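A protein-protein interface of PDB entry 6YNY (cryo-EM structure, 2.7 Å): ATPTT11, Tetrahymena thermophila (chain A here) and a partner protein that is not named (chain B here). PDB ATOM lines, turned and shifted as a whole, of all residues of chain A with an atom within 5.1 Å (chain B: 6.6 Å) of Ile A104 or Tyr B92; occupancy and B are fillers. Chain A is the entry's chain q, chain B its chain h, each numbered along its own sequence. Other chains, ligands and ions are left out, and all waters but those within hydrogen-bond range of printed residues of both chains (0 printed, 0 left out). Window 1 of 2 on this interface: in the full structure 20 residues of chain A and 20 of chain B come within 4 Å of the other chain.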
ATOM      1  N   GLU A 100     -32.696   4.759  17.894  1.00  0.00           N
ATOM      2  CA  GLU A 100     -31.327   4.816  18.391  1.00  0.00           C
ATOM      3  C   GLU A 100     -31.190   4.103  19.727  1.00  0.00           C
ATOM      4  O   GLU A 100     -30.173   3.451  19.990  1.00  0.00           O
ATOM      5  CB  GLU A 100     -30.881   6.272  18.513  1.00  0.00           C
ATOM      6  CG  GLU A 100     -31.683   7.091  19.506  1.00  0.00           C
ATOM      7  CD  GLU A 100     -31.190   8.519  19.620  1.00  0.00           C
ATOM      8  OE1 GLU A 100     -30.320   8.918  18.819  1.00  0.00           O
ATOM      9  OE2 GLU A 100     -31.670   9.245  20.515  1.00  0.00           O
ATOM     10  N   PHE A 101     -32.202   4.213  20.587  1.00  0.00           N
ATOM     11  CA  PHE A 101     -32.127   3.584  21.897  1.00  0.00           C
ATOM     12  C   PHE A 101     -32.249   2.073  21.810  1.00  0.00           C
ATOM     13  O   PHE A 101     -31.777   1.372  22.711  1.00  0.00           O
ATOM     14  CB  PHE A 101     -33.208   4.154  22.812  1.00  0.00           C
ATOM     15  CG  PHE A 101     -33.102   5.631  23.017  1.00  0.00           C
ATOM     16  CD1 PHE A 101     -32.050   6.166  23.732  1.00  0.00           C
ATOM     17  CD2 PHE A 101     -34.053   6.485  22.497  1.00  0.00           C
ATOM     18  CE1 PHE A 101     -31.946   7.520  23.920  1.00  0.00           C
ATOM     19  CE2 PHE A 101     -33.953   7.842  22.685  1.00  0.00           C
ATOM     20  CZ  PHE A 101     -32.899   8.359  23.398  1.00  0.00           C
ATOM     21  N   ASP A 102     -32.867   1.557  20.751  1.00  0.00           N
ATOM     22  CA  ASP A 102     -32.971   0.115  20.580  1.00  0.00           C
ATOM     23  C   ASP A 102     -31.673  -0.484  20.070  1.00  0.00           C
ATOM     24  O   ASP A 102     -31.357  -1.634  20.393  1.00  0.00           O
ATOM     25  CB  ASP A 102     -34.116  -0.219  19.628  1.00  0.00           C
ATOM     26  CG  ASP A 102     -35.474   0.071  20.226  1.00  0.00           C
ATOM     27  OD1 ASP A 102     -35.626  -0.075  21.455  1.00  0.00           O
ATOM     28  OD2 ASP A 102     -36.391   0.447  19.469  1.00  0.00           O
ATOM     29  N   SER A 103     -30.913   0.271  19.277  1.00  0.00           N
ATOM     30  CA  SER A 103     -29.608  -0.202  18.836  1.00  0.00           C
ATOM     31  C   SER A 103     -28.657  -0.369  20.010  1.00  0.00           C
ATOM     32  O   SER A 103     -27.773  -1.233  19.977  1.00  0.00           O
ATOM     33  CB  SER A 103     -29.020   0.764  17.814  1.00  0.00           C
ATOM     34  OG  SER A 103     -29.815   0.815  16.648  1.00  0.00           O
ATOM     35  N   ILE A 104     -28.818   0.446  21.051  1.00  0.00           N
ATOM     36  CA  ILE A 104     -28.000   0.297  22.247  1.00  0.00           C
ATOM     37  C   ILE A 104     -28.302  -1.032  22.927  1.00  0.00           C
ATOM     38  O   ILE A 104     -27.392  -1.801  23.254  1.00  0.00           O
ATOM     39  CB  ILE A 104     -28.228   1.486  23.196  1.00  0.00           C
ATOM     40  CG1 ILE A 104     -27.920   2.801  22.484  1.00  0.00           C
ATOM     41  CG2 ILE A 104     -27.363   1.360  24.430  1.00  0.00           C
ATOM     42  CD1 ILE A 104     -28.364   4.024  23.242  1.00  0.00           C
ATOM     43  N   GLU A 105     -29.585  -1.323  23.145  1.00  0.00           N
ATOM     44  CA  GLU A 105     -29.964  -2.589  23.760  1.00  0.00           C
ATOM     45  C   GLU A 105     -29.454  -3.775  22.955  1.00  0.00           C
ATOM     46  O   GLU A 105     -29.116  -4.815  23.528  1.00  0.00           O
ATOM     47  CB  GLU A 105     -31.481  -2.665  23.901  1.00  0.00           C
ATOM     48  CG  GLU A 105     -32.060  -1.723  24.931  1.00  0.00           C
ATOM     49  CD  GLU A 105     -31.735  -2.134  26.350  1.00  0.00           C
ATOM     50  OE1 GLU A 105     -31.102  -3.194  26.535  1.00  0.00           O
ATOM     51  OE2 GLU A 105     -32.116  -1.397  27.283  1.00  0.00           O
ATOM     52  N   LEU A 106     -29.406  -3.641  21.631  1.00  0.00           N
ATOM     53  CA  LEU A 106     -28.872  -4.709  20.795  1.00  0.00           C
ATOM     54  C   LEU A 106     -27.367  -4.839  20.973  1.00  0.00           C
ATOM     55  O   LEU A 106     -26.841  -5.948  21.120  1.00  0.00           O
ATOM     56  CB  LEU A 106     -29.218  -4.444  19.334  1.00  0.00           C
ATOM     57  CG  LEU A 106     -30.698  -4.516  18.972  1.00  0.00           C
ATOM     58  CD1 LEU A 106     -30.923  -3.995  17.577  1.00  0.00           C
ATOM     59  CD2 LEU A 106     -31.197  -5.933  19.088  1.00  0.00           C
ATOM     60  N   ALA A 107     -26.655  -3.714  20.959  1.00  0.00           N
ATOM     61  CA  ALA A 107     -25.219  -3.748  21.203  1.00  0.00           C
ATOM     62  C   ALA A 107     -24.914  -4.279  22.595  1.00  0.00           C
ATOM     63  O   ALA A 107     -23.977  -5.063  22.778  1.00  0.00           O
ATOM     64  CB  ALA A 107     -24.630  -2.354  21.022  1.00  0.00           C
ATOM     65  N   MET A 108     -25.696  -3.863  23.591  1.00  0.00           N
ATOM     66  CA  MET A 108     -25.521  -4.395  24.936  1.00  0.00           C
ATOM     67  C   MET A 108     -25.659  -5.908  24.951  1.00  0.00           C
ATOM     68  O   MET A 108     -25.023  -6.584  25.766  1.00  0.00           O
ATOM     69  CB  MET A 108     -26.538  -3.761  25.882  1.00  0.00           C
ATOM     70  CG  MET A 108     -26.347  -2.279  26.089  1.00  0.00           C
ATOM     71  SD  MET A 108     -27.780  -1.484  26.827  1.00  0.00           S
ATOM     72  CE  MET A 108     -27.854  -2.353  28.380  1.00  0.00           C
ATOM     73  N   GLN A 109     -26.485  -6.456  24.062  1.00  0.00           N
ATOM     74  CA  GLN A 109     -26.649  -7.899  23.986  1.00  0.00           C
ATOM     75  C   GLN A 109     -25.488  -8.556  23.256  1.00  0.00           C
ATOM     76  O   GLN A 109     -25.162  -9.714  23.531  1.00  0.00           O
ATOM     77  CB  GLN A 109     -27.965  -8.233  23.291  1.00  0.00           C
ATOM     78  CG  GLN A 109     -28.366  -9.679  23.402  1.00  0.00           C
ATOM     79  CD  GLN A 109     -28.672 -10.087  24.824  1.00  0.00           C
ATOM     80  OE1 GLN A 109     -29.040  -9.258  25.654  1.00  0.00           O
ATOM     81  NE2 GLN A 109     -28.517 -11.368  25.115  1.00  0.00           N
ATOM     82  N   ILE A 123     -21.671   2.738  18.908  1.00  0.00           N
ATOM     83  CA  ILE A 123     -23.067   2.302  18.909  1.00  0.00           C
ATOM     84  C   ILE A 123     -23.923   3.115  17.947  1.00  0.00           C
ATOM     85  O   ILE A 123     -24.675   2.512  17.164  1.00  0.00           O
ATOM     86  CB  ILE A 123     -23.620   2.327  20.345  1.00  0.00           C
ATOM     87  CG1 ILE A 123     -22.818   1.377  21.234  1.00  0.00           C
ATOM     88  CG2 ILE A 123     -25.084   1.967  20.336  1.00  0.00           C
ATOM     89  CD1 ILE A 123     -23.170   1.438  22.691  1.00  0.00           C
ATOM     90  N   ARG B  87     -22.400  11.083  25.880  1.00  0.00           N
ATOM     91  CA  ARG B  87     -22.830  10.948  27.265  1.00  0.00           C
ATOM     92  C   ARG B  87     -24.299  10.560  27.353  1.00  0.00           C
ATOM     93  O   ARG B  87     -24.708   9.892  28.309  1.00  0.00           O
ATOM     94  CB  ARG B  87     -22.569  12.251  28.018  1.00  0.00           C
ATOM     95  CG  ARG B  87     -21.150  12.407  28.505  1.00  0.00           C
ATOM     96  CD  ARG B  87     -20.766  13.855  28.725  1.00  0.00           C
ATOM     97  NE  ARG B  87     -21.745  14.595  29.512  1.00  0.00           N
ATOM     98  CZ  ARG B  87     -21.898  14.467  30.824  1.00  0.00           C
ATOM     99  NH1 ARG B  87     -21.146  13.616  31.502  1.00  0.00           N
ATOM    100  NH2 ARG B  87     -22.811  15.187  31.455  1.00  0.00           N
ATOM    101  N   TYR B  88     -25.102  10.964  26.369  1.00  0.00           N
ATOM    102  CA  TYR B  88     -26.500  10.556  26.328  1.00  0.00           C
ATOM    103  C   TYR B  88     -26.632   9.082  25.975  1.00  0.00           C
ATOM    104  O   TYR B  88     -27.619   8.440  26.346  1.00  0.00           O
ATOM    105  CB  TYR B  88     -27.249  11.421  25.316  1.00  0.00           C
ATOM    106  CG  TYR B  88     -28.733  11.565  25.554  1.00  0.00           C
ATOM    107  CD1 TYR B  88     -29.649  10.848  24.804  1.00  0.00           C
ATOM    108  CD2 TYR B  88     -29.217  12.434  26.516  1.00  0.00           C
ATOM    109  CE1 TYR B  88     -31.006  10.988  25.017  1.00  0.00           C
ATOM    110  CE2 TYR B  88     -30.566  12.577  26.735  1.00  0.00           C
ATOM    111  CZ  TYR B  88     -31.458  11.855  25.985  1.00  0.00           C
ATOM    112  OH  TYR B  88     -32.804  12.007  26.209  1.00  0.00           O
ATOM    113  N   VAL B  89     -25.646   8.533  25.269  1.00  0.00           N
ATOM    114  CA  VAL B  89     -25.684   7.135  24.863  1.00  0.00           C
ATOM    115  C   VAL B  89     -25.210   6.235  25.993  1.00  0.00           C
ATOM    116  O   VAL B  89     -25.855   5.236  26.326  1.00  0.00           O
ATOM    117  CB  VAL B  89     -24.837   6.938  23.594  1.00  0.00           C
ATOM    118  CG1 VAL B  89     -24.685   5.472  23.270  1.00  0.00           C
ATOM    119  CG2 VAL B  89     -25.456   7.675  22.431  1.00  0.00           C
ATOM    120  N   GLN B  90     -24.068   6.571  26.591  1.00  0.00           N
ATOM    121  CA  GLN B  90     -23.533   5.757  27.672  1.00  0.00           C
ATOM    122  C   GLN B  90     -24.429   5.805  28.899  1.00  0.00           C
ATOM    123  O   GLN B  90     -24.552   4.807  29.616  1.00  0.00           O
ATOM    124  CB  GLN B  90     -22.124   6.225  28.020  1.00  0.00           C
ATOM    125  CG  GLN B  90     -21.401   5.340  29.001  1.00  0.00           C
ATOM    126  CD  GLN B  90     -21.158   3.952  28.464  1.00  0.00           C
ATOM    127  OE1 GLN B  90     -20.962   3.761  27.267  1.00  0.00           O
ATOM    128  NE2 GLN B  90     -21.180   2.970  29.350  1.00  0.00           N
ATOM    129  N   THR B  91     -25.061   6.949  29.155  1.00  0.00           N
ATOM    130  CA  THR B  91     -25.965   7.055  30.292  1.00  0.00           C
ATOM    131  C   THR B  91     -27.121   6.074  30.164  1.00  0.00           C
ATOM    132  O   THR B  91     -27.549   5.473  31.155  1.00  0.00           O
ATOM    133  CB  THR B  91     -26.479   8.488  30.410  1.00  0.00           C
ATOM    134  OG1 THR B  91     -25.387   9.367  30.697  1.00  0.00           O
ATOM    135  CG2 THR B  91     -27.508   8.598  31.501  1.00  0.00           C
ATOM    136  N   TYR B  92     -27.643   5.900  28.949  1.00  0.00           N
ATOM    137  CA  TYR B  92     -28.696   4.918  28.728  1.00  0.00           C
ATOM    138  C   TYR B  92     -28.188   3.507  28.984  1.00  0.00           C
ATOM    139  O   TYR B  92     -28.825   2.723  29.694  1.00  0.00           O
ATOM    140  CB  TYR B  92     -29.228   5.045  27.303  1.00  0.00           C
ATOM    141  CG  TYR B  92     -30.394   4.141  26.998  1.00  0.00           C
ATOM    142  CD1 TYR B  92     -31.695   4.587  27.143  1.00  0.00           C
ATOM    143  CD2 TYR B  92     -30.195   2.844  26.562  1.00  0.00           C
ATOM    144  CE1 TYR B  92     -32.760   3.769  26.866  1.00  0.00           C
ATOM    145  CE2 TYR B  92     -31.254   2.020  26.286  1.00  0.00           C
ATOM    146  CZ  TYR B  92     -32.536   2.487  26.438  1.00  0.00           C
ATOM    147  OH  TYR B  92     -33.598   1.665  26.160  1.00  0.00           O
ATOM    148  N   ARG B  93     -27.034   3.168  28.409  1.00  0.00           N
ATOM    149  CA  ARG B  93     -26.490   1.827  28.570  1.00  0.00           C
ATOM    150  C   ARG B  93     -26.264   1.498  30.038  1.00  0.00           C
ATOM    151  O   ARG B  93     -26.476   0.358  30.467  1.00  0.00           O
ATOM    152  CB  ARG B  93     -25.187   1.702  27.789  1.00  0.00           C
ATOM    153  CG  ARG B  93     -24.658   0.297  27.688  1.00  0.00           C
ATOM    154  CD  ARG B  93     -23.233   0.200  28.155  1.00  0.00           C
ATOM    155  NE  ARG B  93     -22.334   1.051  27.385  1.00  0.00           N
ATOM    156  CZ  ARG B  93     -21.727   0.687  26.262  1.00  0.00           C
ATOM    157  NH1 ARG B  93     -21.914  -0.517  25.751  1.00  0.00           N
ATOM    158  NH2 ARG B  93     -20.928   1.537  25.645  1.00  0.00           N
ATOM    159  N   ASN B  94     -25.833   2.482  30.823  1.00  0.00           N
ATOM    160  CA  ASN B  94     -25.579   2.240  32.238  1.00  0.00           C
ATOM    161  C   ASN B  94     -26.882   2.086  33.010  1.00  0.00           C
ATOM    162  O   ASN B  94     -27.068   1.112  33.747  1.00  0.00           O
ATOM    163  CB  ASN B  94     -24.744   3.376  32.819  1.00  0.00           C
ATOM    164  CG  ASN B  94     -23.412   3.532  32.132  1.00  0.00           C
ATOM    165  OD1 ASN B  94     -22.908   2.606  31.502  1.00  0.00           O
ATOM    166  ND2 ASN B  94     -22.826   4.709  32.265  1.00  0.00           N
ATOM    167  N   MET B  95     -27.795   3.044  32.857  1.00  0.00           N
ATOM    168  CA  MET B  95     -29.050   2.990  33.594  1.00  0.00           C
ATOM    169  C   MET B  95     -29.823   1.718  33.280  1.00  0.00           C
ATOM    170  O   MET B  95     -30.543   1.201  34.140  1.00  0.00           O
ATOM    171  CB  MET B  95     -29.889   4.223  33.272  1.00  0.00           C
ATOM    172  CG  MET B  95     -29.215   5.514  33.675  1.00  0.00           C
ATOM    173  SD  MET B  95     -29.956   6.990  32.970  1.00  0.00           S
ATOM    174  CE  MET B  95     -31.424   7.130  33.963  1.00  0.00           C
ATOM    175  N   SER B  96     -29.684   1.200  32.062  1.00  0.00           N
ATOM    176  CA  SER B  96     -30.351  -0.043  31.701  1.00  0.00           C
ATOM    177  C   SER B  96     -29.646  -1.242  32.314  1.00  0.00           C
ATOM    178  O   SER B  96     -30.279  -2.090  32.948  1.00  0.00           O
ATOM    179  CB  SER B  96     -30.406  -0.181  30.183  1.00  0.00           C
ATOM    180  OG  SER B  96     -31.000  -1.409  29.807  1.00  0.00           O
ATOM    181  N   ARG B  97     -28.328  -1.318  32.137  1.00  0.00           N
ATOM    182  CA  ARG B  97     -27.580  -2.479  32.598  1.00  0.00           C
ATOM    183  C   ARG B  97     -27.499  -2.537  34.117  1.00  0.00           C
ATOM    184  O   ARG B  97     -27.505  -3.629  34.693  1.00  0.00           O
ATOM    185  CB  ARG B  97     -26.185  -2.455  31.985  1.00  0.00           C
ATOM    186  CG  ARG B  97     -25.313  -3.609  32.362  1.00  0.00           C
ATOM    187  CD  ARG B  97     -24.062  -3.608  31.534  1.00  0.00           C
ATOM    188  NE  ARG B  97     -24.324  -3.971  30.149  1.00  0.00           N
ATOM    189  CZ  ARG B  97     -23.473  -3.770  29.152  1.00  0.00           C
ATOM    190  NH1 ARG B  97     -23.795  -4.136  27.925  1.00  0.00           N
ATOM    191  NH2 ARG B  97     -22.308  -3.187  29.376  1.00  0.00           N
ATOM    192  N   PHE B 113     -39.335  -2.403  31.851  1.00  0.00           N
ATOM    193  CA  PHE B 113     -38.433  -1.347  32.290  1.00  0.00           C
ATOM    194  C   PHE B 113     -37.870  -0.569  31.109  1.00  0.00           C
ATOM    195  O   PHE B 113     -37.692   0.651  31.187  1.00  0.00           O
ATOM    196  CB  PHE B 113     -37.308  -1.952  33.123  1.00  0.00           C
ATOM    197  CG  PHE B 113     -36.106  -1.077  33.245  1.00  0.00           C
ATOM    198  CD1 PHE B 113     -36.075  -0.040  34.152  1.00  0.00           C
ATOM    199  CD2 PHE B 113     -35.000  -1.300  32.454  1.00  0.00           C
ATOM    200  CE1 PHE B 113     -34.967   0.760  34.260  1.00  0.00           C
ATOM    201  CE2 PHE B 113     -33.895  -0.504  32.559  1.00  0.00           C
ATOM    202  CZ  PHE B 113     -33.875   0.527  33.463  1.00  0.00           C
ATOM    203  N   ILE B 114     -37.584  -1.257  30.004  1.00  0.00           N
ATOM    204  CA  ILE B 114     -37.063  -0.577  28.822  1.00  0.00           C
ATOM    205  C   ILE B 114     -38.067   0.453  28.323  1.00  0.00           C
ATOM    206  O   ILE B 114     -37.714   1.601  28.035  1.00  0.00           O
ATOM    207  CB  ILE B 114     -36.713  -1.601  27.730  1.00  0.00           C
ATOM    208  CG1 ILE B 114     -35.476  -2.398  28.132  1.00  0.00           C
ATOM    209  CG2 ILE B 114     -36.486  -0.909  26.409  1.00  0.00           C
ATOM    210  CD1 ILE B 114     -35.251  -3.631  27.305  1.00  0.00           C
ATOM    211  N   LEU B 115     -39.334   0.055  28.213  1.00  0.00           N
ATOM    212  CA  LEU B 115     -40.366   0.994  27.795  1.00  0.00           C
ATOM    213  C   LEU B 115     -40.417   2.202  28.719  1.00  0.00           C
ATOM    214  O   LEU B 115     -40.635   3.332  28.266  1.00  0.00           O
ATOM    215  CB  LEU B 115     -41.718   0.290  27.764  1.00  0.00           C
ATOM    216  CG  LEU B 115     -41.814  -0.899  26.815  1.00  0.00           C
ATOM    217  CD1 LEU B 115     -43.144  -1.585  26.964  1.00  0.00           C
ATOM    218  CD2 LEU B 115     -41.611  -0.462  25.391  1.00  0.00           C
ATOM    219  N   LEU B 117     -37.828   3.293  30.577  1.00  0.00           N
ATOM    220  CA  LEU B 117     -36.581   4.026  30.417  1.00  0.00           C
ATOM    221  C   LEU B 117     -36.616   4.903  29.174  1.00  0.00           C
ATOM    222  O   LEU B 117     -36.089   6.020  29.181  1.00  0.00           O
ATOM    223  CB  LEU B 117     -35.417   3.045  30.354  1.00  0.00           C
ATOM    224  CG  LEU B 117     -34.012   3.630  30.394  1.00  0.00           C
ATOM    225  CD1 LEU B 117     -33.768   4.343  31.699  1.00  0.00           C
ATOM    226  CD2 LEU B 117     -33.000   2.533  30.191  1.00  0.00           C
ATOM    227  N   ARG B 118     -37.236   4.417  28.099  1.00  0.00           N
ATOM    228  CA  ARG B 118     -37.334   5.218  26.885  1.00  0.00           C
ATOM    229  C   ARG B 118     -38.224   6.433  27.100  1.00  0.00           C
ATOM    230  O   ARG B 118     -37.928   7.522  26.595  1.00  0.00           O
ATOM    231  CB  ARG B 118     -37.862   4.363  25.738  1.00  0.00           C
ATOM    232  CG  ARG B 118     -36.931   3.242  25.352  1.00  0.00           C
ATOM    233  CD  ARG B 118     -37.493   2.368  24.248  1.00  0.00           C
ATOM    234  NE  ARG B 118     -37.550   3.060  22.964  1.00  0.00           N
ATOM    235  CZ  ARG B 118     -38.634   3.634  22.458  1.00  0.00           C
ATOM    236  NH1 ARG B 118     -39.789   3.612  23.111  1.00  0.00           N
ATOM    237  NH2 ARG B 118     -38.562   4.233  21.282  1.00  0.00           N
ATOM    238  N   PHE B 121     -36.012   9.127  28.405  1.00  0.00           N
ATOM    239  CA  PHE B 121     -35.059   9.703  27.470  1.00  0.00           C
ATOM    240  C   PHE B 121     -35.724  10.408  26.298  1.00  0.00           C
ATOM    241  O   PHE B 121     -35.074  11.227  25.639  1.00  0.00           O
ATOM    242  CB  PHE B 121     -34.131   8.612  26.931  1.00  0.00           C
ATOM    243  CG  PHE B 121     -33.071   8.190  27.899  1.00  0.00           C
ATOM    244  CD1 PHE B 121     -31.748   8.512  27.682  1.00  0.00           C
ATOM    245  CD2 PHE B 121     -33.398   7.476  29.031  1.00  0.00           C
ATOM    246  CE1 PHE B 121     -30.779   8.128  28.570  1.00  0.00           C
ATOM    247  CE2 PHE B 121     -32.429   7.093  29.920  1.00  0.00           C
ATOM    248  CZ  PHE B 121     -31.119   7.419  29.690  1.00  0.00           C
ATOM    249  N   LEU B 146     -29.800  13.365  33.720  1.00  0.00           N
ATOM    250  CA  LEU B 146     -29.838  11.909  33.715  1.00  0.00           C
ATOM    251  C   LEU B 146     -28.677  11.316  34.496  1.00  0.00           C
ATOM    252  O   LEU B 146     -28.808  10.234  35.076  1.00  0.00           O
ATOM    253  CB  LEU B 146     -29.819  11.401  32.277  1.00  0.00           C
ATOM    254  CG  LEU B 146     -31.017  11.806  31.428  1.00  0.00           C
ATOM    255  CD1 LEU B 146     -30.726  11.581  29.965  1.00  0.00           C
ATOM    256  CD2 LEU B 146     -32.234  11.027  31.846  1.00  0.00           C
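Of the 18 printed residues of chain B, 9 touch a printed residue of chain A.
Hydrophobic or aromatic side chains of chain B that line the printed part of chain A: Tyr B88, Val B89, Tyr B92, Ile B114 and Phe B121.
Of the 11 printed residues of chain A, 6 touch a printed residue of chain B.
Hydrophobic or aromatic side chains of chain A that line the printed part of chain B: Phe A101, Ile A104, Met A108 and Ile A123.
Among the printed residues, 13 pairs touch across the chains.
Among the printed residues, Asp or Glu carboxylates within 4 Å of a Lys or Arg side-chain nitrogen of the other chain: Asp A102 with Arg B118.
The backbone carbonyl oxygen (O) of Met A108 lies close to the guanidinium group (NH1) of Arg B97.
OD1 of Asp A102 lies within salt-bridge range of NE of Arg B118, 3.98 Å away.
The side-chain carboxylate (OE2) of Glu A105 lies within hydrogen-bond range of the side-chain hydroxyl (OG) of Ser B96, at 2.8 Å.
Of chain A, only Phe A101 (3.7 Å), Ile A104 (3.8 Å) and Glu A105 (3.6 Å) come within 4 Å of Tyr B92.
Printed residues of chain A within 4 Å of Arg B93: Met A108 and Ile A123.
Of the printed residues of chain A, Arg B118 touches Asp A102.
The nearest printed residue of chain B that does not touch Ile A104 is Arg B93 (4.02 Å).
The side-chain amide oxygen of Gln B90 is in hydrogen-bond range of the guanidinium group of Arg B93, at 2.8 Å.
The side-chain hydroxyl of Tyr B88 is in hydrogen-bond range of the backbone carbonyl oxygen of Phe B121 (2.5 Å).
Tyr B88 touches Phe A101.
Phe A101 touches Tyr B92.
Phe A101 touches Phe B121 (CZ to CB, 3.8 Å).
Ile A104 touches Val B89 (CD1 to CG1, 3.95 Å).
Tyr B92 touches Ile A104 (CD2 to CG2, 3.8 Å).
OE2 of Glu A105 touches OH of Tyr B92 (3.6 Å).
OE2 of Glu A105 touches CG1 of Ile B114, 3.6 Å away.
Met A108 touches Arg B93 (CG to CG, 3.5 Å).
CE of Met A108 touches OG of Ser B96 (3.6 Å).
Ile A123 touches Arg B93.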
